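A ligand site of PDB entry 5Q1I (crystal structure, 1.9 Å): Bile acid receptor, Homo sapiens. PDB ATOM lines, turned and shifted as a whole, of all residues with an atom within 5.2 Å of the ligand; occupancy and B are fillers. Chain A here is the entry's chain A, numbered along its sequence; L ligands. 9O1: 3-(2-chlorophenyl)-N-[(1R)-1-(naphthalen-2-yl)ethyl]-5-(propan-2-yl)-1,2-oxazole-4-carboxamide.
OG1 of Thr 49 lies within hydrogen-bond range of O of Phe 45.
The side-chain hydroxyl (OG) of Ser 93 sits at hydrogen-bond distance from the backbone carbonyl oxygen (O) of Met 89 (2.7 Å).
The side-chain hydroxyl (OH) of Tyr 130 lies close to the side-chain sulfur (SD) of Met 126.
O17 of the ligand sits at hydrogen-bond distance from OH of Tyr 130, at 3.1 Å.
The side-chain hydroxyl (OG) of Ser 93 lies within hydrogen-bond range of a nitrogen (N16) of the ligand, 2.8 Å away.
Residues that only touch the ligand: Phe 45, Leu 48, Thr 49, Met 51, Ala 52, His 55, Met 89, Phe 90, Ile 96, Phe 97, Leu 109, Ile 113, Ile 118, Met 126 and Trp 230.
Hydrophobic or aromatic side chains within 4 Å of the ligand: Phe 45, Leu 48, Met 51, Ala 52, His 55, Met 89, Phe 90, Ile 96, Phe 97, Leu 109, Ile 113, Ile 118, Met 126, Tyr 130 and Trp 230.
Within 4 Å of the ligand: Phe 45, Leu 48, Thr 49, Met 51, Ala 52, His 55, Met 89, Phe 90, Ser 93, Ile 96, Phe 97, Leu 109, Ile 113, Ile 118, Met 126, Tyr 130 and Trp 230.
The nearest printed residue that does not touch the ligand is Leu 226 (4.1 Å).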
ATOM      1  N   PHE A  45      -9.286  -1.530  -0.406  1.00  0.00           N
ATOM      2  CA  PHE A  45      -8.845  -0.234   0.125  1.00  0.00           C
ATOM      3  C   PHE A  45      -8.197  -0.352   1.499  1.00  0.00           C
ATOM      4  O   PHE A  45      -7.232   0.349   1.777  1.00  0.00           O
ATOM      5  CB  PHE A  45      -9.988   0.788   0.142  1.00  0.00           C
ATOM      6  CG  PHE A  45      -9.472   2.176   0.442  1.00  0.00           C
ATOM      7  CD1 PHE A  45      -8.917   2.964  -0.570  1.00  0.00           C
ATOM      8  CD2 PHE A  45      -9.474   2.671   1.739  1.00  0.00           C
ATOM      9  CE1 PHE A  45      -8.400   4.225  -0.286  1.00  0.00           C
ATOM     10  CE2 PHE A  45      -8.942   3.926   2.029  1.00  0.00           C
ATOM     11  CZ  PHE A  45      -8.417   4.704   1.012  1.00  0.00           C
ATOM     12  N   LEU A  48      -4.698  -1.428   1.067  1.00  0.00           N
ATOM     13  CA  LEU A  48      -3.936  -0.237   0.634  1.00  0.00           C
ATOM     14  C   LEU A  48      -3.572   0.632   1.837  1.00  0.00           C
ATOM     15  O   LEU A  48      -2.423   1.101   1.939  1.00  0.00           O
ATOM     16  CB  LEU A  48      -4.719   0.609  -0.379  1.00  0.00           C
ATOM     17  CG  LEU A  48      -5.051  -0.015  -1.744  1.00  0.00           C
ATOM     18  CD1 LEU A  48      -5.541   1.044  -2.693  1.00  0.00           C
ATOM     19  CD2 LEU A  48      -3.851  -0.694  -2.329  1.00  0.00           C
ATOM     20  N   THR A  49      -4.551   0.861   2.742  1.00  0.00           N
ATOM     21  CA  THR A  49      -4.414   1.639   3.980  1.00  0.00           C
ATOM     22  C   THR A  49      -3.303   1.038   4.857  1.00  0.00           C
ATOM     23  O   THR A  49      -2.422   1.762   5.308  1.00  0.00           O
ATOM     24  CB  THR A  49      -5.775   1.685   4.723  1.00  0.00           C
ATOM     25  OG1 THR A  49      -6.697   2.381   3.910  1.00  0.00           O
ATOM     26  CG2 THR A  49      -5.675   2.384   6.094  1.00  0.00           C
ATOM     27  N   MET A  51      -0.859  -0.930   3.925  1.00  0.00           N
ATOM     28  CA  MET A  51       0.406  -0.771   3.208  1.00  0.00           C
ATOM     29  C   MET A  51       0.973   0.648   3.386  1.00  0.00           C
ATOM     30  O   MET A  51       2.170   0.807   3.627  1.00  0.00           O
ATOM     31  CB  MET A  51       0.242  -1.145   1.740  1.00  0.00           C
ATOM     32  CG  MET A  51       0.023  -2.628   1.569  1.00  0.00           C
ATOM     33  SD  MET A  51      -0.103  -3.074  -0.151  1.00  0.00           S
ATOM     34  CE  MET A  51       1.692  -3.023  -0.586  1.00  0.00           C
ATOM     35  N   ALA A  52       0.099   1.671   3.325  1.00  0.00           N
ATOM     36  CA  ALA A  52       0.442   3.085   3.545  1.00  0.00           C
ATOM     37  C   ALA A  52       0.939   3.330   4.979  1.00  0.00           C
ATOM     38  O   ALA A  52       1.921   4.045   5.148  1.00  0.00           O
ATOM     39  CB  ALA A  52      -0.753   3.971   3.236  1.00  0.00           C
ATOM     40  N   HIS A  55       4.408   1.697   5.220  1.00  0.00           N
ATOM     41  CA  HIS A  55       5.391   2.525   4.496  1.00  0.00           C
ATOM     42  C   HIS A  55       5.840   3.763   5.282  1.00  0.00           C
ATOM     43  O   HIS A  55       7.033   4.049   5.275  1.00  0.00           O
ATOM     44  CB  HIS A  55       4.926   2.904   3.080  1.00  0.00           C
ATOM     45  CG  HIS A  55       5.972   3.702   2.350  1.00  0.00           C
ATOM     46  ND1 HIS A  55       5.857   5.071   2.215  1.00  0.00           N
ATOM     47  CD2 HIS A  55       7.191   3.318   1.885  1.00  0.00           C
ATOM     48  CE1 HIS A  55       6.977   5.475   1.629  1.00  0.00           C
ATOM     49  NE2 HIS A  55       7.801   4.452   1.390  1.00  0.00           N
ATOM     50  N   MET A  89       6.397   7.455  -1.110  1.00  0.00           N
ATOM     51  CA  MET A  89       5.486   6.312  -1.271  1.00  0.00           C
ATOM     52  C   MET A  89       5.320   5.928  -2.749  1.00  0.00           C
ATOM     53  O   MET A  89       5.357   4.737  -3.075  1.00  0.00           O
ATOM     54  CB  MET A  89       4.132   6.597  -0.601  1.00  0.00           C
ATOM     55  CG  MET A  89       3.141   5.495  -0.785  1.00  0.00           C
ATOM     56  SD  MET A  89       1.478   5.849  -0.212  1.00  0.00           S
ATOM     57  CE  MET A  89       1.043   7.198  -1.327  1.00  0.00           C
ATOM     58  N   PHE A  90       5.158   6.930  -3.630  1.00  0.00           N
ATOM     59  CA  PHE A  90       5.036   6.668  -5.073  1.00  0.00           C
ATOM     60  C   PHE A  90       6.336   6.122  -5.646  1.00  0.00           C
ATOM     61  O   PHE A  90       6.301   5.311  -6.564  1.00  0.00           O
ATOM     62  CB  PHE A  90       4.612   7.929  -5.842  1.00  0.00           C
ATOM     63  CG  PHE A  90       3.122   8.171  -5.804  1.00  0.00           C
ATOM     64  CD1 PHE A  90       2.287   7.592  -6.742  1.00  0.00           C
ATOM     65  CD2 PHE A  90       2.560   8.975  -4.812  1.00  0.00           C
ATOM     66  CE1 PHE A  90       0.898   7.781  -6.680  1.00  0.00           C
ATOM     67  CE2 PHE A  90       1.183   9.177  -4.766  1.00  0.00           C
ATOM     68  CZ  PHE A  90       0.356   8.579  -5.695  1.00  0.00           C
ATOM     69  N   ARG A  92       8.614   4.260  -3.988  1.00  0.00           N
ATOM     70  CA  ARG A  92       8.709   2.894  -3.491  1.00  0.00           C
ATOM     71  C   ARG A  92       7.720   1.994  -4.256  1.00  0.00           C
ATOM     72  O   ARG A  92       8.078   0.875  -4.601  1.00  0.00           O
ATOM     73  CB  ARG A  92       8.458   2.842  -1.968  1.00  0.00           C
ATOM     74  CG  ARG A  92       8.385   1.448  -1.322  1.00  0.00           C
ATOM     75  CD  ARG A  92       9.663   0.621  -1.460  1.00  0.00           C
ATOM     76  NE  ARG A  92       9.481  -0.700  -0.848  1.00  0.00           N
ATOM     77  CZ  ARG A  92      10.090  -1.815  -1.239  1.00  0.00           C
ATOM     78  NH1 ARG A  92      10.927  -1.793  -2.273  1.00  0.00           N
ATOM     79  NH2 ARG A  92       9.852  -2.961  -0.616  1.00  0.00           N
ATOM     80  N   SER A  93       6.514   2.506  -4.540  1.00  0.00           N
ATOM     81  CA  SER A  93       5.473   1.819  -5.327  1.00  0.00           C
ATOM     82  C   SER A  93       5.968   1.536  -6.738  1.00  0.00           C
ATOM     83  O   SER A  93       5.729   0.444  -7.245  1.00  0.00           O
ATOM     84  CB  SER A  93       4.207   2.651  -5.384  1.00  0.00           C
ATOM     85  OG  SER A  93       3.674   2.828  -4.075  1.00  0.00           O
ATOM     86  N   ILE A  96       8.401  -1.449  -6.323  1.00  0.00           N
ATOM     87  CA  ILE A  96       7.618  -2.677  -6.118  1.00  0.00           C
ATOM     88  C   ILE A  96       7.015  -3.180  -7.460  1.00  0.00           C
ATOM     89  O   ILE A  96       7.085  -4.377  -7.742  1.00  0.00           O
ATOM     90  CB  ILE A  96       6.525  -2.471  -5.024  1.00  0.00           C
ATOM     91  CG1 ILE A  96       7.144  -2.335  -3.614  1.00  0.00           C
ATOM     92  CG2 ILE A  96       5.448  -3.578  -5.045  1.00  0.00           C
ATOM     93  CD1 ILE A  96       6.189  -1.713  -2.572  1.00  0.00           C
ATOM     94  N   PHE A  97       6.443  -2.268  -8.277  1.00  0.00           N
ATOM     95  CA  PHE A  97       5.846  -2.601  -9.567  1.00  0.00           C
ATOM     96  C   PHE A  97       6.851  -3.177 -10.562  1.00  0.00           C
ATOM     97  O   PHE A  97       6.529  -4.132 -11.274  1.00  0.00           O
ATOM     98  CB  PHE A  97       5.145  -1.375 -10.195  1.00  0.00           C
ATOM     99  CG  PHE A  97       4.488  -1.620 -11.536  1.00  0.00           C
ATOM    100  CD1 PHE A  97       3.204  -2.138 -11.614  1.00  0.00           C
ATOM    101  CD2 PHE A  97       5.173  -1.351 -12.727  1.00  0.00           C
ATOM    102  CE1 PHE A  97       2.609  -2.388 -12.860  1.00  0.00           C
ATOM    103  CE2 PHE A  97       4.564  -1.584 -13.969  1.00  0.00           C
ATOM    104  CZ  PHE A  97       3.289  -2.109 -14.029  1.00  0.00           C
ATOM    105  N   SER A 106       2.182  -9.970  -7.244  1.00  0.00           N
ATOM    106  CA  SER A 106       2.153  -8.634  -7.837  1.00  0.00           C
ATOM    107  C   SER A 106       0.927  -8.349  -8.686  1.00  0.00           C
ATOM    108  O   SER A 106       0.384  -7.255  -8.622  1.00  0.00           O
ATOM    109  CB  SER A 106       3.433  -8.375  -8.642  1.00  0.00           C
ATOM    110  OG  SER A 106       3.575  -9.292  -9.707  1.00  0.00           O
ATOM    111  N   LEU A 109      -2.045  -7.899  -6.302  1.00  0.00           N
ATOM    112  CA  LEU A 109      -1.962  -6.577  -5.676  1.00  0.00           C
ATOM    113  C   LEU A 109      -2.398  -5.478  -6.661  1.00  0.00           C
ATOM    114  O   LEU A 109      -3.196  -4.637  -6.277  1.00  0.00           O
ATOM    115  CB  LEU A 109      -0.556  -6.319  -5.091  1.00  0.00           C
ATOM    116  CG  LEU A 109      -0.262  -4.933  -4.455  1.00  0.00           C
ATOM    117  CD1 LEU A 109      -1.269  -4.570  -3.353  1.00  0.00           C
ATOM    118  CD2 LEU A 109       1.153  -4.892  -3.913  1.00  0.00           C
ATOM    119  N   GLU A 110      -1.926  -5.540  -7.920  1.00  0.00           N
ATOM    120  CA  GLU A 110      -2.336  -4.583  -8.950  1.00  0.00           C
ATOM    121  C   GLU A 110      -3.848  -4.630  -9.172  1.00  0.00           C
ATOM    122  O   GLU A 110      -4.473  -3.584  -9.302  1.00  0.00           O
ATOM    123  CB  GLU A 110      -1.587  -4.828 -10.271  1.00  0.00           C
ATOM    124  CG  GLU A 110      -2.110  -3.926 -11.393  1.00  0.00           C
ATOM    125  CD  GLU A 110      -1.323  -3.845 -12.675  1.00  0.00           C
ATOM    126  OE1 GLU A 110      -0.220  -4.432 -12.749  1.00  0.00           O
ATOM    127  OE2 GLU A 110      -1.786  -3.138 -13.599  1.00  0.00           O
ATOM    128  N   ILE A 113      -5.564  -2.758  -6.222  1.00  0.00           N
ATOM    129  CA  ILE A 113      -5.428  -1.289  -6.373  1.00  0.00           C
ATOM    130  C   ILE A 113      -6.416  -0.728  -7.400  1.00  0.00           C
ATOM    131  O   ILE A 113      -7.019   0.320  -7.173  1.00  0.00           O
ATOM    132  CB  ILE A 113      -3.957  -0.877  -6.653  1.00  0.00           C
ATOM    133  CG1 ILE A 113      -3.084  -1.245  -5.461  1.00  0.00           C
ATOM    134  CG2 ILE A 113      -3.829   0.628  -6.944  1.00  0.00           C
ATOM    135  CD1 ILE A 113      -1.797  -1.645  -5.774  1.00  0.00           C
ATOM    136  N   ILE A 118     -10.892   3.778  -5.916  1.00  0.00           N
ATOM    137  CA  ILE A 118     -10.164   4.970  -6.332  1.00  0.00           C
ATOM    138  C   ILE A 118     -10.422   5.206  -7.824  1.00  0.00           C
ATOM    139  O   ILE A 118     -10.319   4.273  -8.621  1.00  0.00           O
ATOM    140  CB  ILE A 118      -8.659   4.898  -6.013  1.00  0.00           C
ATOM    141  CG1 ILE A 118      -8.407   4.643  -4.511  1.00  0.00           C
ATOM    142  CG2 ILE A 118      -7.917   6.165  -6.511  1.00  0.00           C
ATOM    143  CD1 ILE A 118      -7.001   4.228  -4.187  1.00  0.00           C
ATOM    144  N   MET A 126      -0.718   7.060 -12.176  1.00  0.00           N
ATOM    145  CA  MET A 126       0.004   6.237 -11.203  1.00  0.00           C
ATOM    146  C   MET A 126       0.783   5.129 -11.960  1.00  0.00           C
ATOM    147  O   MET A 126       2.006   5.119 -11.920  1.00  0.00           O
ATOM    148  CB  MET A 126      -1.026   5.650 -10.228  1.00  0.00           C
ATOM    149  CG  MET A 126      -0.478   5.166  -8.921  1.00  0.00           C
ATOM    150  SD  MET A 126      -1.766   4.390  -7.901  1.00  0.00           S
ATOM    151  CE  MET A 126      -2.787   5.817  -7.535  1.00  0.00           C
ATOM    152  N   PHE A 127       0.066   4.261 -12.720  1.00  0.00           N
ATOM    153  CA  PHE A 127       0.709   3.172 -13.489  1.00  0.00           C
ATOM    154  C   PHE A 127       1.541   3.687 -14.654  1.00  0.00           C
ATOM    155  O   PHE A 127       2.562   3.075 -14.981  1.00  0.00           O
ATOM    156  CB  PHE A 127      -0.306   2.100 -13.936  1.00  0.00           C
ATOM    157  CG  PHE A 127      -0.707   1.250 -12.754  1.00  0.00           C
ATOM    158  CD1 PHE A 127      -1.810   1.599 -11.972  1.00  0.00           C
ATOM    159  CD2 PHE A 127       0.061   0.158 -12.373  1.00  0.00           C
ATOM    160  CE1 PHE A 127      -2.143   0.843 -10.847  1.00  0.00           C
ATOM    161  CE2 PHE A 127      -0.277  -0.582 -11.234  1.00  0.00           C
ATOM    162  CZ  PHE A 127      -1.370  -0.241 -10.487  1.00  0.00           C
ATOM    163  N   TYR A 130       4.851   4.377 -13.090  1.00  0.00           N
ATOM    164  CA  TYR A 130       5.575   3.138 -12.792  1.00  0.00           C
ATOM    165  C   TYR A 130       6.228   2.585 -14.052  1.00  0.00           C
ATOM    166  O   TYR A 130       7.358   2.113 -13.991  1.00  0.00           O
ATOM    167  CB  TYR A 130       4.639   2.074 -12.195  1.00  0.00           C
ATOM    168  CG  TYR A 130       3.919   2.454 -10.905  1.00  0.00           C
ATOM    169  CD1 TYR A 130       4.375   3.500 -10.114  1.00  0.00           C
ATOM    170  CD2 TYR A 130       2.788   1.765 -10.498  1.00  0.00           C
ATOM    171  CE1 TYR A 130       3.697   3.865  -8.947  1.00  0.00           C
ATOM    172  CE2 TYR A 130       2.100   2.121  -9.351  1.00  0.00           C
ATOM    173  CZ  TYR A 130       2.555   3.173  -8.567  1.00  0.00           C
ATOM    174  OH  TYR A 130       1.872   3.512  -7.435  1.00  0.00           O
ATOM    175  N   HIS A 208      -2.593  13.557  -5.396  1.00  0.00           N
ATOM    176  CA  HIS A 208      -2.882  12.775  -4.192  1.00  0.00           C
ATOM    177  C   HIS A 208      -3.687  13.574  -3.143  1.00  0.00           C
ATOM    178  O   HIS A 208      -4.594  13.018  -2.522  1.00  0.00           O
ATOM    179  CB  HIS A 208      -1.571  12.274  -3.577  1.00  0.00           C
ATOM    180  CG  HIS A 208      -1.749  11.138  -2.634  1.00  0.00           C
ATOM    181  ND1 HIS A 208      -1.859   9.849  -3.084  1.00  0.00           N
ATOM    182  CD2 HIS A 208      -1.819  11.150  -1.283  1.00  0.00           C
ATOM    183  CE1 HIS A 208      -1.997   9.098  -1.999  1.00  0.00           C
ATOM    184  NE2 HIS A 208      -1.984   9.848  -0.894  1.00  0.00           N
ATOM    185  N   MET A 211      -7.229  13.981  -4.378  1.00  0.00           N
ATOM    186  CA  MET A 211      -7.893  12.682  -4.219  1.00  0.00           C
ATOM    187  C   MET A 211      -8.401  12.510  -2.776  1.00  0.00           C
ATOM    188  O   MET A 211      -9.532  12.058  -2.560  1.00  0.00           O
ATOM    189  CB  MET A 211      -6.911  11.553  -4.590  1.00  0.00           C
ATOM    190  CG  MET A 211      -7.487  10.146  -4.439  1.00  0.00           C
ATOM    191  SD  MET A 211      -6.260   8.814  -4.609  1.00  0.00           S
ATOM    192  CE  MET A 211      -5.357   8.991  -3.098  1.00  0.00           C
ATOM    193  N   TRP A 215     -12.769  12.545  -0.728  1.00  0.00           N
ATOM    194  CA  TRP A 215     -13.422  11.483   0.030  1.00  0.00           C
ATOM    195  C   TRP A 215     -14.315  12.020   1.140  1.00  0.00           C
ATOM    196  O   TRP A 215     -13.843  12.701   2.052  1.00  0.00           O
ATOM    197  CB  TRP A 215     -12.409  10.463   0.583  1.00  0.00           C
ATOM    198  CG  TRP A 215     -11.495   9.830  -0.439  1.00  0.00           C
ATOM    199  CD1 TRP A 215     -11.692   9.756  -1.794  1.00  0.00           C
ATOM    200  CD2 TRP A 215     -10.256   9.168  -0.181  1.00  0.00           C
ATOM    201  NE1 TRP A 215     -10.626   9.136  -2.395  1.00  0.00           N
ATOM    202  CE2 TRP A 215      -9.732   8.741  -1.427  1.00  0.00           C
ATOM    203  CE3 TRP A 215      -9.504   8.907   0.981  1.00  0.00           C
ATOM    204  CZ2 TRP A 215      -8.509   8.060  -1.540  1.00  0.00           C
ATOM    205  CZ3 TRP A 215      -8.287   8.255   0.867  1.00  0.00           C
ATOM    206  CH2 TRP A 215      -7.806   7.831  -0.373  1.00  0.00           C
ATOM    207  N   LEU A 226      -4.761   8.513   7.617  1.00  0.00           N
ATOM    208  CA  LEU A 226      -4.144   8.824   6.322  1.00  0.00           C
ATOM    209  C   LEU A 226      -4.057  10.335   6.106  1.00  0.00           C
ATOM    210  O   LEU A 226      -3.017  10.818   5.661  1.00  0.00           O
ATOM    211  CB  LEU A 226      -4.891   8.145   5.145  1.00  0.00           C
ATOM    212  CG  LEU A 226      -4.784   6.618   5.027  1.00  0.00           C
ATOM    213  CD1 LEU A 226      -5.518   6.108   3.782  1.00  0.00           C
ATOM    214  CD2 LEU A 226      -3.330   6.128   5.056  1.00  0.00           C
ATOM    215  N   TRP A 230      -0.490  12.564   5.270  1.00  0.00           N
ATOM    216  CA  TRP A 230      -0.468  13.145   3.930  1.00  0.00           C
ATOM    217  C   TRP A 230      -0.946  14.592   3.775  1.00  0.00           C
ATOM    218  O   TRP A 230      -0.454  15.263   2.867  1.00  0.00           O
ATOM    219  CB  TRP A 230      -1.259  12.258   2.974  1.00  0.00           C
ATOM    220  CG  TRP A 230      -0.753  10.854   2.820  1.00  0.00           C
ATOM    221  CD1 TRP A 230       0.530  10.415   2.949  1.00  0.00           C
ATOM    222  CD2 TRP A 230      -1.518   9.728   2.384  1.00  0.00           C
ATOM    223  NE1 TRP A 230       0.604   9.066   2.682  1.00  0.00           N
ATOM    224  CE2 TRP A 230      -0.634   8.630   2.313  1.00  0.00           C
ATOM    225  CE3 TRP A 230      -2.869   9.525   2.067  1.00  0.00           C
ATOM    226  CZ2 TRP A 230      -1.059   7.358   1.905  1.00  0.00           C
ATOM    227  CZ3 TRP A 230      -3.286   8.282   1.657  1.00  0.00           C
ATOM    228  CH2 TRP A 230      -2.393   7.206   1.591  1.00  0.00           C
HETATM  229  C4  9O1 L   1       3.464   1.207  -1.497  1.00  0.00           C
HETATM  230  C5  9O1 L   1       3.550   1.929  -0.317  1.00  0.00           C
HETATM  231  C6  9O1 L   1       2.408   2.205   0.406  1.00  0.00           C
HETATM  232  C7  9O1 L   1       2.166  -0.004  -3.241  1.00  0.00           C
HETATM  233  C10 9O1 L   1       1.836  -0.776  -5.301  1.00  0.00           C
HETATM  234  C13 9O1 L   1       2.630  -0.749  -7.688  1.00  0.00           C
HETATM  235  C15 9O1 L   1       0.748   1.512  -4.929  1.00  0.00           C
HETATM  236  C20 9O1 L   1      -1.064   4.145  -3.589  1.00  0.00           C
HETATM  237  C21 9O1 L   1       1.155   5.034  -4.425  1.00  0.00           C
HETATM  238  C22 9O1 L   1      -2.181   4.772  -4.166  1.00  0.00           C
HETATM  239  C24 9O1 L   1      -1.107   3.815  -2.256  1.00  0.00           C
HETATM  240  C26 9O1 L   1      -3.380   4.702  -2.057  1.00  0.00           C
HETATM  241  C28 9O1 L   1      -4.550   4.612   0.071  1.00  0.00           C
HETATM  242  C12 9O1 L   1       1.519  -1.158  -6.790  1.00  0.00           C
HETATM  243  C14 9O1 L   1       1.362  -2.666  -6.974  1.00  0.00           C
HETATM  244  O9  9O1 L   1       2.579  -1.662  -4.609  1.00  0.00           O
HETATM  245  N8  9O1 L   1       2.778  -1.172  -3.295  1.00  0.00           N
HETATM  246  C3  9O1 L   1       2.213   0.753  -1.974  1.00  0.00           C
HETATM  247  C1  9O1 L   1       1.168   1.770  -0.042  1.00  0.00           C
HETATM  248  C2  9O1 L   1       1.082   1.048  -1.222  1.00  0.00           C
HETATM  249 CL18 9O1 L   1      -0.475   0.536  -1.734  1.00  0.00          CL
HETATM  250  C11 9O1 L   1       1.546   0.305  -4.505  1.00  0.00           C
HETATM  251  O17 9O1 L   1       0.034   1.478  -5.925  1.00  0.00           O
HETATM  252  N16 9O1 L   1       0.868   2.624  -4.170  1.00  0.00           N
HETATM  253  C19 9O1 L   1       0.160   3.890  -4.459  1.00  0.00           C
HETATM  254  C23 9O1 L   1      -3.308   5.041  -3.438  1.00  0.00           C
HETATM  255  C27 9O1 L   1      -4.529   4.954  -1.262  1.00  0.00           C
HETATM  256  C29 9O1 L   1      -3.447   3.996   0.659  1.00  0.00           C
HETATM  257  C30 9O1 L   1      -2.320   3.734  -0.077  1.00  0.00           C
HETATM  258  C25 9O1 L   1      -2.254   4.078  -1.452  1.00  0.00           C
